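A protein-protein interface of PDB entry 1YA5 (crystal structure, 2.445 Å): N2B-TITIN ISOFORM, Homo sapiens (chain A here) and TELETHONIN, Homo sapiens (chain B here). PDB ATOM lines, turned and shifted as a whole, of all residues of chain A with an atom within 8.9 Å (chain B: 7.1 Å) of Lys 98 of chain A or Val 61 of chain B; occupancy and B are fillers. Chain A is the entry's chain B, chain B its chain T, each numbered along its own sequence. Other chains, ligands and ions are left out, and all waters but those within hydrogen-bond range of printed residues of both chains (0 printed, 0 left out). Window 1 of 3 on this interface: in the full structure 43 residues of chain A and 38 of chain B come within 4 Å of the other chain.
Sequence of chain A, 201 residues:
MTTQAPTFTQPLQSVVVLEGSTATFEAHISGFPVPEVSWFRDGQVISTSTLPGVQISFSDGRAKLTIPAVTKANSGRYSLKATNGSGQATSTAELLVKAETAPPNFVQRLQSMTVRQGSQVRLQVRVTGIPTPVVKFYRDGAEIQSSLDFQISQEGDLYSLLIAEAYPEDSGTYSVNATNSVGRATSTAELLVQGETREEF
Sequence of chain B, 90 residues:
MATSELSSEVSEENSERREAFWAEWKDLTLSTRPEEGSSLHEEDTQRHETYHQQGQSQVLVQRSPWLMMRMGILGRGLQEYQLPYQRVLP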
ATOM      1  N   VAL A  15      21.789   0.546   5.165  1.00  0.00           N
ATOM      2  CA  VAL A  15      20.576   1.202   5.600  1.00  0.00           C
ATOM      3  C   VAL A  15      19.444   0.220   5.940  1.00  0.00           C
ATOM      4  O   VAL A  15      19.315  -0.866   5.351  1.00  0.00           O
ATOM      5  CB  VAL A  15      20.117   2.276   4.602  1.00  0.00           C
ATOM      6  CG1 VAL A  15      21.194   3.308   4.412  1.00  0.00           C
ATOM      7  CG2 VAL A  15      19.738   1.657   3.258  1.00  0.00           C
ATOM      8  N   VAL A  16      18.641   0.605   6.927  1.00  0.00           N
ATOM      9  CA  VAL A  16      17.489  -0.188   7.349  1.00  0.00           C
ATOM     10  C   VAL A  16      16.276   0.696   7.258  1.00  0.00           C
ATOM     11  O   VAL A  16      16.216   1.737   7.907  1.00  0.00           O
ATOM     12  CB  VAL A  16      17.616  -0.668   8.791  1.00  0.00           C
ATOM     13  CG1 VAL A  16      16.594  -1.759   9.060  1.00  0.00           C
ATOM     14  CG2 VAL A  16      18.993  -1.204   9.018  1.00  0.00           C
ATOM     15  N   VAL A  17      15.309   0.279   6.443  1.00  0.00           N
ATOM     16  CA  VAL A  17      14.181   1.146   6.144  1.00  0.00           C
ATOM     17  C   VAL A  17      12.876   0.386   6.117  1.00  0.00           C
ATOM     18  O   VAL A  17      12.864  -0.838   5.959  1.00  0.00           O
ATOM     19  CB  VAL A  17      14.386   1.921   4.823  1.00  0.00           C
ATOM     20  CG1 VAL A  17      15.459   2.971   5.016  1.00  0.00           C
ATOM     21  CG2 VAL A  17      14.780   0.973   3.681  1.00  0.00           C
ATOM     22  N   LEU A  18      11.790   1.139   6.269  1.00  0.00           N
ATOM     23  CA  LEU A  18      10.458   0.594   6.325  1.00  0.00           C
ATOM     24  C   LEU A  18       9.963   0.349   4.916  1.00  0.00           C
ATOM     25  O   LEU A  18      10.117   1.215   4.048  1.00  0.00           O
ATOM     26  CB  LEU A  18       9.556   1.614   6.987  1.00  0.00           C
ATOM     27  CG  LEU A  18       8.424   1.185   7.921  1.00  0.00           C
ATOM     28  CD1 LEU A  18       7.155   1.897   7.476  1.00  0.00           C
ATOM     29  CD2 LEU A  18       8.234  -0.311   7.953  1.00  0.00           C
ATOM     30  N   GLU A  19       9.345  -0.809   4.681  1.00  0.00           N
ATOM     31  CA  GLU A  19       8.768  -1.099   3.373  1.00  0.00           C
ATOM     32  C   GLU A  19       7.897   0.048   2.911  1.00  0.00           C
ATOM     33  O   GLU A  19       7.039   0.509   3.663  1.00  0.00           O
ATOM     34  CB  GLU A  19       7.921  -2.356   3.436  1.00  0.00           C
ATOM     35  CG  GLU A  19       7.860  -3.109   2.130  1.00  0.00           C
ATOM     36  CD  GLU A  19       7.004  -4.357   2.216  1.00  0.00           C
ATOM     37  OE1 GLU A  19       6.726  -4.807   3.348  1.00  0.00           O
ATOM     38  OE2 GLU A  19       6.610  -4.887   1.147  1.00  0.00           O
ATOM     39  N   GLY A  20       8.108   0.499   1.679  1.00  0.00           N
ATOM     40  CA  GLY A  20       7.291   1.549   1.079  1.00  0.00           C
ATOM     41  C   GLY A  20       7.801   2.947   1.335  1.00  0.00           C
ATOM     42  O   GLY A  20       7.161   3.935   0.997  1.00  0.00           O
ATOM     43  N   SER A  21       8.967   3.037   1.946  1.00  0.00           N
ATOM     44  CA  SER A  21       9.573   4.324   2.194  1.00  0.00           C
ATOM     45  C   SER A  21      10.831   4.460   1.344  1.00  0.00           C
ATOM     46  O   SER A  21      11.252   3.517   0.683  1.00  0.00           O
ATOM     47  CB  SER A  21       9.912   4.450   3.678  1.00  0.00           C
ATOM     48  OG  SER A  21      10.826   3.441   4.055  1.00  0.00           O
ATOM     49  N   VAL A  70      10.611   1.609  -1.337  1.00  0.00           N
ATOM     50  CA  VAL A  70      11.338   0.348  -1.344  1.00  0.00           C
ATOM     51  C   VAL A  70      10.379  -0.802  -1.168  1.00  0.00           C
ATOM     52  O   VAL A  70       9.260  -0.621  -0.707  1.00  0.00           O
ATOM     53  CB  VAL A  70      12.353   0.272  -0.208  1.00  0.00           C
ATOM     54  CG1 VAL A  70      13.554   1.088  -0.531  1.00  0.00           C
ATOM     55  CG2 VAL A  70      11.731   0.763   1.077  1.00  0.00           C
ATOM     56  N   THR A  71      10.827  -1.994  -1.529  1.00  0.00           N
ATOM     57  CA  THR A  71       9.994  -3.176  -1.403  1.00  0.00           C
ATOM     58  C   THR A  71      10.894  -4.195  -0.806  1.00  0.00           C
ATOM     59  O   THR A  71      12.105  -4.091  -0.953  1.00  0.00           O
ATOM     60  CB  THR A  71       9.613  -3.726  -2.762  1.00  0.00           C
ATOM     61  OG1 THR A  71      10.781  -4.316  -3.353  1.00  0.00           O
ATOM     62  CG2 THR A  71       9.081  -2.617  -3.675  1.00  0.00           C
ATOM     63  N   LYS A  72      10.313  -5.180  -0.142  1.00  0.00           N
ATOM     64  CA  LYS A  72      11.081  -6.299   0.361  1.00  0.00           C
ATOM     65  C   LYS A  72      11.966  -6.867  -0.751  1.00  0.00           C
ATOM     66  O   LYS A  72      13.059  -7.357  -0.501  1.00  0.00           O
ATOM     67  CB  LYS A  72      10.128  -7.382   0.838  1.00  0.00           C
ATOM     68  CG  LYS A  72      10.560  -8.043   2.112  1.00  0.00           C
ATOM     69  CD  LYS A  72      10.025  -7.297   3.304  1.00  0.00           C
ATOM     70  CE  LYS A  72      10.584  -7.898   4.572  1.00  0.00           C
ATOM     71  NZ  LYS A  72      12.066  -8.056   4.479  1.00  0.00           N
ATOM     72  N   ALA A  73      11.494  -6.802  -1.985  1.00  0.00           N
ATOM     73  CA  ALA A  73      12.242  -7.374  -3.086  1.00  0.00           C
ATOM     74  C   ALA A  73      13.585  -6.685  -3.213  1.00  0.00           C
ATOM     75  O   ALA A  73      14.600  -7.318  -3.497  1.00  0.00           O
ATOM     76  CB  ALA A  73      11.462  -7.227  -4.368  1.00  0.00           C
ATOM     77  N   SER A  75      15.615  -5.723  -1.208  1.00  0.00           N
ATOM     78  CA  SER A  75      16.618  -6.044  -0.189  1.00  0.00           C
ATOM     79  C   SER A  75      17.840  -6.713  -0.784  1.00  0.00           C
ATOM     80  O   SER A  75      17.718  -7.640  -1.584  1.00  0.00           O
ATOM     81  CB  SER A  75      16.043  -6.993   0.850  1.00  0.00           C
ATOM     82  OG  SER A  75      15.910  -6.353   2.100  1.00  0.00           O
ATOM     83  N   LEU A  95      21.078  -3.001   1.862  1.00  0.00           N
ATOM     84  CA  LEU A  95      19.768  -2.433   2.044  1.00  0.00           C
ATOM     85  C   LEU A  95      18.929  -3.510   2.716  1.00  0.00           C
ATOM     86  O   LEU A  95      18.784  -4.611   2.179  1.00  0.00           O
ATOM     87  CB  LEU A  95      19.181  -2.094   0.694  1.00  0.00           C
ATOM     88  CG  LEU A  95      17.724  -1.707   0.700  1.00  0.00           C
ATOM     89  CD1 LEU A  95      17.536  -0.469   1.551  1.00  0.00           C
ATOM     90  CD2 LEU A  95      17.303  -1.455  -0.758  1.00  0.00           C
ATOM     91  N   LEU A  96      18.415  -3.189   3.904  1.00  0.00           N
ATOM     92  CA  LEU A  96      17.650  -4.131   4.714  1.00  0.00           C
ATOM     93  C   LEU A  96      16.222  -3.644   4.826  1.00  0.00           C
ATOM     94  O   LEU A  96      15.972  -2.596   5.403  1.00  0.00           O
ATOM     95  CB  LEU A  96      18.264  -4.220   6.102  1.00  0.00           C
ATOM     96  CG  LEU A  96      19.711  -4.698   6.061  1.00  0.00           C
ATOM     97  CD1 LEU A  96      20.430  -4.229   7.270  1.00  0.00           C
ATOM     98  CD2 LEU A  96      19.825  -6.229   5.919  1.00  0.00           C
ATOM     99  N   VAL A  97      15.276  -4.376   4.254  1.00  0.00           N
ATOM    100  CA  VAL A  97      13.892  -3.894   4.257  1.00  0.00           C
ATOM    101  C   VAL A  97      13.025  -4.582   5.279  1.00  0.00           C
ATOM    102  O   VAL A  97      12.863  -5.810   5.244  1.00  0.00           O
ATOM    103  CB  VAL A  97      13.219  -3.988   2.892  1.00  0.00           C
ATOM    104  CG1 VAL A  97      11.975  -3.118   2.883  1.00  0.00           C
ATOM    105  CG2 VAL A  97      14.196  -3.563   1.805  1.00  0.00           C
ATOM    106  N   LYS A  98      12.482  -3.781   6.190  1.00  0.00           N
ATOM    107  CA  LYS A  98      11.636  -4.288   7.263  1.00  0.00           C
ATOM    108  C   LYS A  98      10.158  -4.117   6.945  1.00  0.00           C
ATOM    109  O   LYS A  98       9.718  -3.033   6.570  1.00  0.00           O
ATOM    110  CB  LYS A  98      11.960  -3.590   8.579  1.00  0.00           C
ATOM    111  CG  LYS A  98      13.378  -3.793   9.028  1.00  0.00           C
ATOM    112  CD  LYS A  98      13.758  -5.256   8.918  1.00  0.00           C
ATOM    113  CE  LYS A  98      15.202  -5.457   9.323  1.00  0.00           C
ATOM    114  NZ  LYS A  98      15.633  -6.848   9.043  1.00  0.00           N
ATOM    115  N   ALA A  99       9.405  -5.204   7.085  1.00  0.00           N
ATOM    116  CA  ALA A  99       7.956  -5.167   6.929  1.00  0.00           C
ATOM    117  C   ALA A  99       7.361  -4.364   8.072  1.00  0.00           C
ATOM    118  O   ALA A  99       7.912  -4.350   9.168  1.00  0.00           O
ATOM    119  CB  ALA A  99       7.391  -6.576   6.943  1.00  0.00           C
ATOM    120  N   GLU A 100       6.244  -3.702   7.845  1.00  0.00           N
ATOM    121  CA  GLU A 100       5.655  -2.997   8.961  1.00  0.00           C
ATOM    122  C   GLU A 100       4.797  -3.930   9.801  1.00  0.00           C
ATOM    123  O   GLU A 100       4.019  -4.747   9.283  1.00  0.00           O
ATOM    124  CB  GLU A 100       4.918  -1.721   8.540  1.00  0.00           C
ATOM    125  CG  GLU A 100       3.700  -1.879   7.675  1.00  0.00           C
ATOM    126  CD  GLU A 100       3.042  -0.535   7.396  1.00  0.00           C
ATOM    127  OE1 GLU A 100       3.503   0.488   7.932  1.00  0.00           O
ATOM    128  OE2 GLU A 100       2.061  -0.486   6.648  1.00  0.00           O
ATOM    129  N   THR A 101       4.988  -3.818  11.114  1.00  0.00           N
ATOM    130  CA  THR A 101       4.323  -4.665  12.080  1.00  0.00           C
ATOM    131  C   THR A 101       4.124  -3.867  13.362  1.00  0.00           C
ATOM    132  O   THR A 101       4.830  -2.899  13.599  1.00  0.00           O
ATOM    133  CB  THR A 101       5.135  -5.956  12.378  1.00  0.00           C
ATOM    134  OG1 THR A 101       6.190  -5.643  13.287  1.00  0.00           O
ATOM    135  CG2 THR A 101       5.722  -6.508  11.129  1.00  0.00           C
ATOM    136  N   VAL A 182       3.558 -10.673  16.403  1.00  0.00           N
ATOM    137  CA  VAL A 182       4.509 -10.025  17.269  1.00  0.00           C
ATOM    138  C   VAL A 182       3.889  -9.552  18.564  1.00  0.00           C
ATOM    139  O   VAL A 182       4.124  -8.420  19.005  1.00  0.00           O
ATOM    140  CB  VAL A 182       5.187  -8.860  16.556  1.00  0.00           C
ATOM    141  CG1 VAL A 182       5.505  -9.250  15.137  1.00  0.00           C
ATOM    142  CG2 VAL A 182       4.304  -7.643  16.563  1.00  0.00           C
ATOM    143  N   SER B   4      19.345 -10.571  19.201  1.00  0.00           N
ATOM    144  CA  SER B   4      18.783 -10.537  20.544  1.00  0.00           C
ATOM    145  C   SER B   4      17.350 -10.125  20.403  1.00  0.00           C
ATOM    146  O   SER B   4      17.045  -9.193  19.670  1.00  0.00           O
ATOM    147  CB  SER B   4      19.505  -9.526  21.437  1.00  0.00           C
ATOM    148  OG  SER B   4      20.915  -9.589  21.268  1.00  0.00           O
ATOM    149  N   GLU B   5      16.473 -10.814  21.116  1.00  0.00           N
ATOM    150  CA  GLU B   5      15.050 -10.535  21.063  1.00  0.00           C
ATOM    151  C   GLU B   5      14.605 -10.039  22.433  1.00  0.00           C
ATOM    152  O   GLU B   5      14.631 -10.781  23.400  1.00  0.00           O
ATOM    153  CB  GLU B   5      14.274 -11.812  20.675  1.00  0.00           C
ATOM    154  CG  GLU B   5      13.479 -11.722  19.367  1.00  0.00           C
ATOM    155  CD  GLU B   5      12.818 -10.343  19.140  1.00  0.00           C
ATOM    156  OE1 GLU B   5      13.045  -9.742  18.062  1.00  0.00           O
ATOM    157  OE2 GLU B   5      12.056  -9.852  20.021  1.00  0.00           O
ATOM    158  N   LYS B  26       6.908  -8.572  21.253  1.00  0.00           N
ATOM    159  CA  LYS B  26       8.244  -8.497  20.690  1.00  0.00           C
ATOM    160  C   LYS B  26       8.537  -7.035  20.484  1.00  0.00           C
ATOM    161  O   LYS B  26       7.965  -6.426  19.593  1.00  0.00           O
ATOM    162  CB  LYS B  26       8.284  -9.224  19.355  1.00  0.00           C
ATOM    163  CG  LYS B  26       8.136 -10.723  19.484  1.00  0.00           C
ATOM    164  CD  LYS B  26       8.091 -11.391  18.109  1.00  0.00           C
ATOM    165  CE  LYS B  26       8.650 -12.818  18.146  1.00  0.00           C
ATOM    166  NZ  LYS B  26       7.618 -13.784  18.591  1.00  0.00           N
ATOM    167  N   ASP B  27       9.396  -6.454  21.313  1.00  0.00           N
ATOM    168  CA  ASP B  27       9.545  -4.991  21.323  1.00  0.00           C
ATOM    169  C   ASP B  27      10.711  -4.540  20.468  1.00  0.00           C
ATOM    170  O   ASP B  27      10.543  -3.750  19.536  1.00  0.00           O
ATOM    171  CB  ASP B  27       9.727  -4.490  22.755  1.00  0.00           C
ATOM    172  CG  ASP B  27      10.050  -3.002  22.834  1.00  0.00           C
ATOM    173  OD1 ASP B  27      10.532  -2.419  21.835  1.00  0.00           O
ATOM    174  OD2 ASP B  27       9.837  -2.403  23.901  1.00  0.00           O
ATOM    175  N   LEU B  28      11.886  -5.040  20.808  1.00  0.00           N
ATOM    176  CA  LEU B  28      13.119  -4.662  20.145  1.00  0.00           C
ATOM    177  C   LEU B  28      13.739  -5.918  19.611  1.00  0.00           C
ATOM    178  O   LEU B  28      13.746  -6.950  20.282  1.00  0.00           O
ATOM    179  CB  LEU B  28      14.081  -4.041  21.147  1.00  0.00           C
ATOM    180  CG  LEU B  28      15.154  -3.060  20.680  1.00  0.00           C
ATOM    181  CD1 LEU B  28      14.677  -2.355  19.453  1.00  0.00           C
ATOM    182  CD2 LEU B  28      15.420  -2.035  21.759  1.00  0.00           C
ATOM    183  N   THR B  29      14.266  -5.833  18.400  1.00  0.00           N
ATOM    184  CA  THR B  29      15.007  -6.934  17.833  1.00  0.00           C
ATOM    185  C   THR B  29      16.364  -6.428  17.333  1.00  0.00           C
ATOM    186  O   THR B  29      16.423  -5.430  16.642  1.00  0.00           O
ATOM    187  CB  THR B  29      14.229  -7.524  16.691  1.00  0.00           C
ATOM    188  OG1 THR B  29      14.801  -8.790  16.333  1.00  0.00           O
ATOM    189  CG2 THR B  29      14.320  -6.589  15.506  1.00  0.00           C
ATOM    190  N   LEU B  30      17.445  -7.121  17.706  1.00  0.00           N
ATOM    191  CA  LEU B  30      18.813  -6.720  17.354  1.00  0.00           C
ATOM    192  C   LEU B  30      19.510  -7.819  16.604  1.00  0.00           C
ATOM    193  O   LEU B  30      19.623  -8.941  17.105  1.00  0.00           O
ATOM    194  CB  LEU B  30      19.628  -6.445  18.613  1.00  0.00           C
ATOM    195  CG  LEU B  30      20.916  -5.644  18.403  1.00  0.00           C
ATOM    196  CD1 LEU B  30      20.632  -4.105  18.325  1.00  0.00           C
ATOM    197  CD2 LEU B  30      21.897  -5.951  19.517  1.00  0.00           C
ATOM    198  N   SER B  31      20.004  -7.520  15.414  1.00  0.00           N
ATOM    199  CA  SER B  31      20.773  -8.536  14.709  1.00  0.00           C
ATOM    200  C   SER B  31      22.137  -8.085  14.234  1.00  0.00           C
ATOM    201  O   SER B  31      22.425  -6.877  14.139  1.00  0.00           O
ATOM    202  CB  SER B  31      19.991  -9.172  13.552  1.00  0.00           C
ATOM    203  OG  SER B  31      19.020  -8.288  13.033  1.00  0.00           O
ATOM    204  N   ARG B  33      24.851  -8.299  11.099  1.00  0.00           N
ATOM    205  CA  ARG B  33      25.064  -8.569   9.683  1.00  0.00           C
ATOM    206  C   ARG B  33      26.517  -8.922   9.419  1.00  0.00           C
ATOM    207  O   ARG B  33      27.425  -8.271   9.933  1.00  0.00           O
ATOM    208  CB  ARG B  33      24.665  -7.373   8.824  1.00  0.00           C
ATOM    209  CG  ARG B  33      23.363  -6.720   9.227  1.00  0.00           C
ATOM    210  CD  ARG B  33      22.178  -7.546   8.796  1.00  0.00           C
ATOM    211  NE  ARG B  33      22.314  -8.002   7.417  1.00  0.00           N
ATOM    212  CZ  ARG B  33      21.863  -9.169   6.975  1.00  0.00           C
ATOM    213  NH1 ARG B  33      21.255  -9.996   7.812  1.00  0.00           N
ATOM    214  NH2 ARG B  33      22.025  -9.513   5.707  1.00  0.00           N
ATOM    215  N   VAL B  59      21.904  -4.197  13.323  1.00  0.00           N
ATOM    216  CA  VAL B  59      20.688  -3.473  13.047  1.00  0.00           C
ATOM    217  C   VAL B  59      19.601  -3.617  14.094  1.00  0.00           C
ATOM    218  O   VAL B  59      19.444  -4.659  14.733  1.00  0.00           O
ATOM    219  CB  VAL B  59      20.153  -3.675  11.614  1.00  0.00           C
ATOM    220  CG1 VAL B  59      20.967  -4.721  10.845  1.00  0.00           C
ATOM    221  CG2 VAL B  59      18.678  -3.986  11.627  1.00  0.00           C
ATOM    222  N   LEU B  60      18.871  -2.528  14.268  1.00  0.00           N
ATOM    223  CA  LEU B  60      17.902  -2.427  15.314  1.00  0.00           C
ATOM    224  C   LEU B  60      16.547  -2.212  14.716  1.00  0.00           C
ATOM    225  O   LEU B  60      16.341  -1.288  13.918  1.00  0.00           O
ATOM    226  CB  LEU B  60      18.254  -1.263  16.225  1.00  0.00           C
ATOM    227  CG  LEU B  60      17.448  -1.140  17.515  1.00  0.00           C
ATOM    228  CD1 LEU B  60      18.428  -0.903  18.613  1.00  0.00           C
ATOM    229  CD2 LEU B  60      16.406   0.004  17.438  1.00  0.00           C
ATOM    230  N   VAL B  61      15.623  -3.087  15.085  1.00  0.00           N
ATOM    231  CA  VAL B  61      14.212  -2.900  14.770  1.00  0.00           C
ATOM    232  C   VAL B  61      13.457  -2.935  16.079  1.00  0.00           C
ATOM    233  O   VAL B  61      13.585  -3.899  16.849  1.00  0.00           O
ATOM    234  CB  VAL B  61      13.640  -3.989  13.830  1.00  0.00           C
ATOM    235  CG1 VAL B  61      12.173  -3.656  13.439  1.00  0.00           C
ATOM    236  CG2 VAL B  61      14.520  -4.151  12.592  1.00  0.00           C
ATOM    237  N   GLN B  62      12.701  -1.863  16.316  1.00  0.00           N
ATOM    238  CA  GLN B  62      11.817  -1.717  17.464  1.00  0.00           C
ATOM    239  C   GLN B  62      10.377  -1.372  17.024  1.00  0.00           C
ATOM    240  O   GLN B  62      10.167  -0.549  16.145  1.00  0.00           O
ATOM    241  CB  GLN B  62      12.356  -0.603  18.342  1.00  0.00           C
ATOM    242  CG  GLN B  62      11.345   0.019  19.235  1.00  0.00           C
ATOM    243  CD  GLN B  62      11.973   0.586  20.461  1.00  0.00           C
ATOM    244  OE1 GLN B  62      12.106  -0.104  21.483  1.00  0.00           O
ATOM    245  NE2 GLN B  62      12.376   1.865  20.386  1.00  0.00           N
ATOM    246  N   ARG B  63       9.395  -2.014  17.650  1.00  0.00           N
ATOM    247  CA  ARG B  63       7.971  -1.788  17.343  1.00  0.00           C
ATOM    248  C   ARG B  63       7.163  -1.575  18.612  1.00  0.00           C
ATOM    249  O   ARG B  63       7.655  -1.762  19.737  1.00  0.00           O
ATOM    250  CB  ARG B  63       7.384  -2.973  16.557  1.00  0.00           C
ATOM    251  CG  ARG B  63       7.515  -4.305  17.271  1.00  0.00           C
ATOM    252  CD  ARG B  63       7.326  -5.520  16.319  1.00  0.00           C
ATOM    253  NE  ARG B  63       8.514  -5.822  15.516  1.00  0.00           N
ATOM    254  CZ  ARG B  63       9.703  -6.107  16.041  1.00  0.00           C
ATOM    255  NH1 ARG B  63       9.840  -6.124  17.351  1.00  0.00           N
ATOM    256  NH2 ARG B  63      10.759  -6.367  15.280  1.00  0.00           N
ATOM    257  N   MET B  69       7.146   2.627  14.801  1.00  0.00           N
ATOM    258  CA  MET B  69       8.334   1.827  14.619  1.00  0.00           C
ATOM    259  C   MET B  69       9.590   2.673  14.693  1.00  0.00           C
ATOM    260  O   MET B  69       9.598   3.896  14.427  1.00  0.00           O
ATOM    261  CB  MET B  69       8.292   1.074  13.303  1.00  0.00           C
ATOM    262  CG  MET B  69       7.649  -0.255  13.430  1.00  0.00           C
ATOM    263  SD  MET B  69       7.758  -1.208  11.947  1.00  0.00           S
ATOM    264  CE  MET B  69       8.867  -2.501  12.547  1.00  0.00           C
ATOM    265  N   ARG B  70      10.661   1.989  15.040  1.00  0.00           N
ATOM    266  CA  ARG B  70      11.936   2.626  15.228  1.00  0.00           C
ATOM    267  C   ARG B  70      12.956   1.623  14.711  1.00  0.00           C
ATOM    268  O   ARG B  70      12.894   0.429  15.044  1.00  0.00           O
ATOM    269  CB  ARG B  70      12.107   2.918  16.705  1.00  0.00           C
ATOM    270  CG  ARG B  70      13.307   3.684  17.056  1.00  0.00           C
ATOM    271  CD  ARG B  70      12.967   5.138  17.321  1.00  0.00           C
ATOM    272  NE  ARG B  70      12.226   5.306  18.562  1.00  0.00           N
ATOM    273  CZ  ARG B  70      12.769   5.656  19.717  1.00  0.00           C
ATOM    274  NH1 ARG B  70      14.084   5.878  19.807  1.00  0.00           N
ATOM    275  NH2 ARG B  70      11.991   5.783  20.790  1.00  0.00           N
ATOM    276  N   MET B  71      13.844   2.084  13.840  1.00  0.00           N
ATOM    277  CA  MET B  71      14.903   1.227  13.290  1.00  0.00           C
ATOM    278  C   MET B  71      16.116   1.993  12.805  1.00  0.00           C
ATOM    279  O   MET B  71      16.074   3.223  12.561  1.00  0.00           O
ATOM    280  CB  MET B  71      14.384   0.342  12.166  1.00  0.00           C
ATOM    281  CG  MET B  71      14.026   1.067  10.903  1.00  0.00           C
ATOM    282  SD  MET B  71      12.876   0.205   9.822  1.00  0.00           S
ATOM    283  CE  MET B  71      11.394   0.042  10.842  1.00  0.00           C
ATOM    284  N   GLY B  72      17.207   1.254  12.674  1.00  0.00           N
ATOM    285  CA  GLY B  72      18.459   1.825  12.214  1.00  0.00           C
ATOM    286  C   GLY B  72      19.658   0.966  12.530  1.00  0.00           C
ATOM    287  O   GLY B  72      19.535  -0.225  12.859  1.00  0.00           O
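The backbone carbonyl oxygen (O) of Val 61 of chain B lies within hydrogen-bond range of the backbone NH (N) of Thr 29 of chain B, 2.6 Å away. The backbone NH of Leu 18 of chain A sits close to the side-chain hydroxyl of Ser 21 of chain A. The backbone carbonyl oxygen (O) of Lys 26 of chain B sits at hydrogen-bond distance from the guanidinium group (NH1) of Arg 63 of chain B, 2.9 Å away. O of Leu 96 of chain A is in hydrogen-bond range of N of Val 17 of chain A. The backbone carbonyl oxygen (O) of Val 17 of chain A sits at hydrogen-bond distance from the backbone NH (N) of Lys 98 of chain A (3.0 Å). The backbone carbonyl oxygen (O) of Val 15 of chain A is in hydrogen-bond range of the backbone NH (N) of Leu 96 of chain A.
Val 61 of chain B touches just one residue of chain A: Lys 98 (3.6 Å). Printed residues of chain B within 4 Å of Val 17 of chain A: Met 71. Of the printed residues of chain A, Met 71 of chain B touches Val 16 (3.8 Å), Val 17 (3.7 Å) and Leu 18 (3.8 Å). Ala 73 of chain A touches none of the printed residues of chain B. Lys 72 of chain A touches none of the printed residues of chain B. The nearest residue of chain A that does not touch Val 61 of chain B is Val 16 of chain A (4.7 Å). The nearest printed residue of chain A that does not touch Arg 63 of chain B is Ala 99 of chain A (6.5 Å).
Val 59 of chain B touches Val 16 of chain A (CB to CG2, 3.8 Å). Val 16 of chain A touches Met 71 of chain B (O to CG, 3.8 Å). SD of Met 71 of chain B touches C of Val 17 of chain A (3.7 Å). Met 71 of chain B touches Leu 18 of chain A. Leu 96 of chain A touches Arg 33 of chain B. Leu 96 of chain A touches Val 59 of chain B. Lys 98 of chain A touches Val 61 of chain B (CE to CG2, 3.6 Å). O of Ala 99 of chain A touches CE of Met 69 of chain B, 3.97 Å away. O of Val 182 of chain A touches N of Lys 26 of chain B, 3.6 Å away. CG2 of Val 182 of chain A touches CD of Arg 63 of chain B, at 3.7 Å.
Of the 18 printed residues of chain B, 7 touch a printed residue of chain A. Hydrophobic or aromatic side chains of chain B that line the printed part of chain A: Val 59, Val 61, Met 69 and Met 71. Along chain B the printed residues that touch a printed residue of chain A span positions 26 to 71. Among the printed residues, 12 pairs touch across the chains.
OG1 of Thr 101 of chain A lies within hydrogen-bond range of NE of Arg 63 of chain B (3.2 Å). The side-chain sulfur (SD) of Met 69 of chain B sits close to the backbone carbonyl oxygen (O) of Thr 101 of chain A, 3.8 Å away.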
